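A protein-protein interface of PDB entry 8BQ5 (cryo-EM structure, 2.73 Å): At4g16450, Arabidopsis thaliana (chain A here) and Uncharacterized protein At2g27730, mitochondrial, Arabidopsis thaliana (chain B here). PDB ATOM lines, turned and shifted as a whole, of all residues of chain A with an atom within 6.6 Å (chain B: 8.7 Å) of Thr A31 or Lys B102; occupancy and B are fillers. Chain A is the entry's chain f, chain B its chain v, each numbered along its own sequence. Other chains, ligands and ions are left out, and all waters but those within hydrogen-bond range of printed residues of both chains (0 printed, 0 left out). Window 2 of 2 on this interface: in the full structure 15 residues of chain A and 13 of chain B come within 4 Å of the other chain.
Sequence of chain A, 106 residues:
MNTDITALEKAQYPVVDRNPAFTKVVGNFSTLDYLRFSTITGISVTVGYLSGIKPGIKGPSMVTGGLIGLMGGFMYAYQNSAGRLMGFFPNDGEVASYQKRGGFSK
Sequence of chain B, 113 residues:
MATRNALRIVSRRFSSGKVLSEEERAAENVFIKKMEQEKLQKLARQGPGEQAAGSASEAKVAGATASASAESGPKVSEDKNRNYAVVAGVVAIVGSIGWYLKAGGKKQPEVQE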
ATOM      1  N   PHE A  29       4.154  -5.982 -15.187  1.00  0.00           N
ATOM      2  CA  PHE A  29       4.527  -6.269 -16.569  1.00  0.00           C
ATOM      3  C   PHE A  29       3.306  -6.683 -17.382  1.00  0.00           C
ATOM      4  O   PHE A  29       2.536  -7.553 -16.968  1.00  0.00           O
ATOM      5  CB  PHE A  29       5.575  -7.383 -16.623  1.00  0.00           C
ATOM      6  CG  PHE A  29       6.971  -6.937 -16.286  1.00  0.00           C
ATOM      7  CD1 PHE A  29       7.244  -5.620 -15.966  1.00  0.00           C
ATOM      8  CD2 PHE A  29       8.016  -7.851 -16.284  1.00  0.00           C
ATOM      9  CE1 PHE A  29       8.530  -5.221 -15.651  1.00  0.00           C
ATOM     10  CE2 PHE A  29       9.302  -7.458 -15.972  1.00  0.00           C
ATOM     11  CZ  PHE A  29       9.560  -6.143 -15.653  1.00  0.00           C
ATOM     12  N   SER A  30       3.140  -6.066 -18.547  1.00  0.00           N
ATOM     13  CA  SER A  30       2.054  -6.395 -19.454  1.00  0.00           C
ATOM     14  C   SER A  30       2.543  -7.388 -20.504  1.00  0.00           C
ATOM     15  O   SER A  30       3.716  -7.763 -20.548  1.00  0.00           O
ATOM     16  CB  SER A  30       1.495  -5.129 -20.106  1.00  0.00           C
ATOM     17  OG  SER A  30       2.515  -4.390 -20.752  1.00  0.00           O
ATOM     18  N   THR A  31       1.623  -7.819 -21.368  1.00  0.00           N
ATOM     19  CA  THR A  31       2.003  -8.709 -22.459  1.00  0.00           C
ATOM     20  C   THR A  31       2.939  -8.010 -23.439  1.00  0.00           C
ATOM     21  O   THR A  31       3.813  -8.651 -24.034  1.00  0.00           O
ATOM     22  CB  THR A  31       0.754  -9.234 -23.168  1.00  0.00           C
ATOM     23  OG1 THR A  31       1.119  -9.860 -24.404  1.00  0.00           O
ATOM     24  CG2 THR A  31      -0.218  -8.110 -23.431  1.00  0.00           C
ATOM     25  N   LEU A  32       2.781  -6.697 -23.617  1.00  0.00           N
ATOM     26  CA  LEU A  32       3.715  -5.952 -24.454  1.00  0.00           C
ATOM     27  C   LEU A  32       5.110  -5.925 -23.836  1.00  0.00           C
ATOM     28  O   LEU A  32       6.114  -6.004 -24.553  1.00  0.00           O
ATOM     29  CB  LEU A  32       3.199  -4.534 -24.686  1.00  0.00           C
ATOM     30  CG  LEU A  32       3.971  -3.700 -25.710  1.00  0.00           C
ATOM     31  CD1 LEU A  32       4.185  -4.478 -27.001  1.00  0.00           C
ATOM     32  CD2 LEU A  32       3.265  -2.383 -25.978  1.00  0.00           C
ATOM     33  N   ASP A  33       5.179  -5.820 -22.505  1.00  0.00           N
ATOM     34  CA  ASP A  33       6.483  -5.830 -21.786  1.00  0.00           C
ATOM     35  C   ASP A  33       7.172  -7.180 -21.985  1.00  0.00           C
ATOM     36  O   ASP A  33       8.385  -7.181 -22.237  1.00  0.00           O
ATOM     37  CB  ASP A  33       6.320  -5.566 -20.287  1.00  0.00           C
ATOM     38  CG  ASP A  33       5.953  -4.137 -19.931  1.00  0.00           C
ATOM     39  OD1 ASP A  33       5.979  -3.278 -20.831  1.00  0.00           O
ATOM     40  OD2 ASP A  33       5.649  -3.898 -18.752  1.00  0.00           O
ATOM     41  N   TYR A  34       6.417  -8.277 -21.880  1.00  0.00           N
ATOM     42  CA  TYR A  34       6.985  -9.637 -22.071  1.00  0.00           C
ATOM     43  C   TYR A  34       7.338  -9.842 -23.546  1.00  0.00           C
ATOM     44  O   TYR A  34       8.297 -10.570 -23.817  1.00  0.00           O
ATOM     45  CB  TYR A  34       6.017 -10.701 -21.560  1.00  0.00           C
ATOM     46  CG  TYR A  34       5.892 -10.789 -20.061  1.00  0.00           C
ATOM     47  CD1 TYR A  34       4.698 -10.492 -19.427  1.00  0.00           C
ATOM     48  CD2 TYR A  34       6.964 -11.179 -19.277  1.00  0.00           C
ATOM     49  CE1 TYR A  34       4.572 -10.571 -18.052  1.00  0.00           C
ATOM     50  CE2 TYR A  34       6.856 -11.261 -17.900  1.00  0.00           C
ATOM     51  CZ  TYR A  34       5.655 -10.957 -17.285  1.00  0.00           C
ATOM     52  OH  TYR A  34       5.535 -11.035 -15.929  1.00  0.00           O
ATOM     53  N   LEU A  35       6.611  -9.194 -24.459  1.00  0.00           N
ATOM     54  CA  LEU A  35       6.938  -9.280 -25.905  1.00  0.00           C
ATOM     55  C   LEU A  35       8.270  -8.574 -26.169  1.00  0.00           C
ATOM     56  O   LEU A  35       9.115  -9.179 -26.843  1.00  0.00           O
ATOM     57  CB  LEU A  35       5.808  -8.656 -26.730  1.00  0.00           C
ATOM     58  CG  LEU A  35       4.626  -9.579 -27.023  1.00  0.00           C
ATOM     59  CD1 LEU A  35       3.429  -8.788 -27.524  1.00  0.00           C
ATOM     60  CD2 LEU A  35       5.012 -10.661 -28.016  1.00  0.00           C
ATOM     61  N   ARG A  36       8.458  -7.365 -25.633  1.00  0.00           N
ATOM     62  CA  ARG A  36       9.724  -6.608 -25.822  1.00  0.00           C
ATOM     63  C   ARG A  36      10.878  -7.420 -25.240  1.00  0.00           C
ATOM     64  O   ARG A  36      11.896  -7.556 -25.931  1.00  0.00           O
ATOM     65  CB  ARG A  36       9.669  -5.264 -25.092  1.00  0.00           C
ATOM     66  CG  ARG A  36       8.528  -4.346 -25.500  1.00  0.00           C
ATOM     67  CD  ARG A  36       8.405  -3.231 -24.483  1.00  0.00           C
ATOM     68  NE  ARG A  36       7.707  -2.057 -24.985  1.00  0.00           N
ATOM     69  CZ  ARG A  36       6.617  -1.537 -24.436  1.00  0.00           C
ATOM     70  NH1 ARG A  36       6.092  -2.084 -23.353  1.00  0.00           N
ATOM     71  NH2 ARG A  36       6.058  -0.469 -24.970  1.00  0.00           N
ATOM     72  N   GLY B  95       7.981 -12.469 -31.705  1.00  0.00           N
ATOM     73  CA  GLY B  95       7.915 -11.370 -30.764  1.00  0.00           C
ATOM     74  C   GLY B  95       7.912 -10.018 -31.443  1.00  0.00           C
ATOM     75  O   GLY B  95       7.230  -9.100 -30.993  1.00  0.00           O
ATOM     76  N   SER B  96       8.678  -9.868 -32.528  1.00  0.00           N
ATOM     77  CA  SER B  96       8.634  -8.618 -33.280  1.00  0.00           C
ATOM     78  C   SER B  96       7.250  -8.388 -33.873  1.00  0.00           C
ATOM     79  O   SER B  96       6.722  -7.268 -33.834  1.00  0.00           O
ATOM     80  CB  SER B  96       9.694  -8.624 -34.382  1.00  0.00           C
ATOM     81  OG  SER B  96      11.002  -8.616 -33.840  1.00  0.00           O
ATOM     82  N   ILE B  97       6.644  -9.446 -34.420  1.00  0.00           N
ATOM     83  CA  ILE B  97       5.301  -9.317 -34.985  1.00  0.00           C
ATOM     84  C   ILE B  97       4.302  -8.918 -33.902  1.00  0.00           C
ATOM     85  O   ILE B  97       3.506  -7.988 -34.080  1.00  0.00           O
ATOM     86  CB  ILE B  97       4.884 -10.620 -35.691  1.00  0.00           C
ATOM     87  CG1 ILE B  97       5.793 -10.895 -36.888  1.00  0.00           C
ATOM     88  CG2 ILE B  97       3.433 -10.544 -36.138  1.00  0.00           C
ATOM     89  CD1 ILE B  97       5.722 -12.320 -37.391  1.00  0.00           C
ATOM     90  N   GLY B  98       4.336  -9.609 -32.761  1.00  0.00           N
ATOM     91  CA  GLY B  98       3.423  -9.276 -31.677  1.00  0.00           C
ATOM     92  C   GLY B  98       3.671  -7.891 -31.109  1.00  0.00           C
ATOM     93  O   GLY B  98       2.731  -7.175 -30.749  1.00  0.00           O
ATOM     94  N   TRP B  99       4.943  -7.494 -31.031  1.00  0.00           N
ATOM     95  CA  TRP B  99       5.309  -6.162 -30.571  1.00  0.00           C
ATOM     96  C   TRP B  99       4.705  -5.095 -31.469  1.00  0.00           C
ATOM     97  O   TRP B  99       4.157  -4.099 -30.985  1.00  0.00           O
ATOM     98  CB  TRP B  99       6.837  -6.053 -30.529  1.00  0.00           C
ATOM     99  CG  TRP B  99       7.402  -4.822 -29.877  1.00  0.00           C
ATOM    100  CD1 TRP B  99       6.733  -3.681 -29.539  1.00  0.00           C
ATOM    101  CD2 TRP B  99       8.766  -4.613 -29.492  1.00  0.00           C
ATOM    102  NE1 TRP B  99       7.595  -2.777 -28.969  1.00  0.00           N
ATOM    103  CE2 TRP B  99       8.850  -3.325 -28.927  1.00  0.00           C
ATOM    104  CE3 TRP B  99       9.926  -5.391 -29.572  1.00  0.00           C
ATOM    105  CZ2 TRP B  99      10.045  -2.799 -28.444  1.00  0.00           C
ATOM    106  CZ3 TRP B  99      11.110  -4.867 -29.090  1.00  0.00           C
ATOM    107  CH2 TRP B  99      11.160  -3.583 -28.533  1.00  0.00           C
ATOM    108  N   TYR B 100       4.791  -5.286 -32.789  1.00  0.00           N
ATOM    109  CA  TYR B 100       4.149  -4.329 -33.685  1.00  0.00           C
ATOM    110  C   TYR B 100       2.633  -4.359 -33.531  1.00  0.00           C
ATOM    111  O   TYR B 100       1.982  -3.308 -33.537  1.00  0.00           O
ATOM    112  CB  TYR B 100       4.545  -4.587 -35.145  1.00  0.00           C
ATOM    113  CG  TYR B 100       3.622  -3.901 -36.143  1.00  0.00           C
ATOM    114  CD1 TYR B 100       4.012  -2.737 -36.790  1.00  0.00           C
ATOM    115  CD2 TYR B 100       2.377  -4.439 -36.468  1.00  0.00           C
ATOM    116  CE1 TYR B 100       3.174  -2.107 -37.692  1.00  0.00           C
ATOM    117  CE2 TYR B 100       1.536  -3.816 -37.355  1.00  0.00           C
ATOM    118  CZ  TYR B 100       1.939  -2.653 -37.972  1.00  0.00           C
ATOM    119  OH  TYR B 100       1.102  -2.039 -38.875  1.00  0.00           O
ATOM    120  N   LEU B 101       2.046  -5.557 -33.437  1.00  0.00           N
ATOM    121  CA  LEU B 101       0.590  -5.659 -33.458  1.00  0.00           C
ATOM    122  C   LEU B 101      -0.034  -5.082 -32.197  1.00  0.00           C
ATOM    123  O   LEU B 101      -1.184  -4.628 -32.221  1.00  0.00           O
ATOM    124  CB  LEU B 101       0.156  -7.112 -33.648  1.00  0.00           C
ATOM    125  CG  LEU B 101       0.287  -7.645 -35.074  1.00  0.00           C
ATOM    126  CD1 LEU B 101      -0.304  -9.040 -35.181  1.00  0.00           C
ATOM    127  CD2 LEU B 101      -0.383  -6.694 -36.053  1.00  0.00           C
ATOM    128  N   LYS B 102       0.696  -5.095 -31.084  1.00  0.00           N
ATOM    129  CA  LYS B 102       0.175  -4.569 -29.830  1.00  0.00           C
ATOM    130  C   LYS B 102       0.867  -3.266 -29.430  1.00  0.00           C
ATOM    131  O   LYS B 102       1.068  -2.996 -28.242  1.00  0.00           O
ATOM    132  CB  LYS B 102       0.288  -5.633 -28.738  1.00  0.00           C
ATOM    133  CG  LYS B 102      -0.489  -5.323 -27.474  1.00  0.00           C
ATOM    134  CD  LYS B 102      -1.372  -6.481 -27.071  1.00  0.00           C
ATOM    135  CE  LYS B 102      -2.007  -6.207 -25.724  1.00  0.00           C
ATOM    136  NZ  LYS B 102      -3.274  -5.443 -25.857  1.00  0.00           N
ATOM    137  N   ALA B 103       1.238  -2.448 -30.407  1.00  0.00           N
ATOM    138  CA  ALA B 103       1.793  -1.131 -30.134  1.00  0.00           C
ATOM    139  C   ALA B 103       1.330  -0.136 -31.194  1.00  0.00           C
ATOM    140  O   ALA B 103       0.229  -0.259 -31.732  1.00  0.00           O
ATOM    141  CB  ALA B 103       3.310  -1.185 -30.078  1.00  0.00           C
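Lys B102 touches Thr A31 (CE to CG2, 3.5 Å). Leu A32 touches Trp B99. Leu A32 touches Lys B102. CD1 of Leu A35 touches O of Gly B98, 3.7 Å away. Arg A36 touches Trp B99.
Of chain B, only Lys B102 comes within 4 Å of Thr A31. Lys B102 touches just these residues of chain A: Thr A31 and Leu A32. Ser A30 touches none of the printed residues of chain B. Leu A32 touches two residues of chain B. Of the printed residues of chain B, Leu A35 touches Gly B98 (3.7 Å). Of the printed residues of chain B, Arg A36 touches Trp B99. Printed residues of chain A within 4 Å of Gly B98: Leu A35. The nearest residue of chain A that does not touch Lys B102 is Leu A35 (4.6 Å).
Printed residues of chain B that touch a printed residue of chain A: Gly B98, Trp B99 and Lys B102. Along chain B the printed residues that touch a printed residue of chain A span positions 98 to 102. Printed residues of chain A that touch a printed residue of chain B: Thr A31, Leu A32, Leu A35 and Arg A36. Hydrophobic or aromatic side chains of chain A that line the printed part of chain B: Leu A32 and Leu A35. Among the printed residues, no Asp or Glu carboxylate lies within 4 Å of a Lys or Arg side-chain nitrogen of the other chain.
OD1 of Asp A33 lies within salt-bridge range of NH1 of Arg A36 (2.8 Å).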
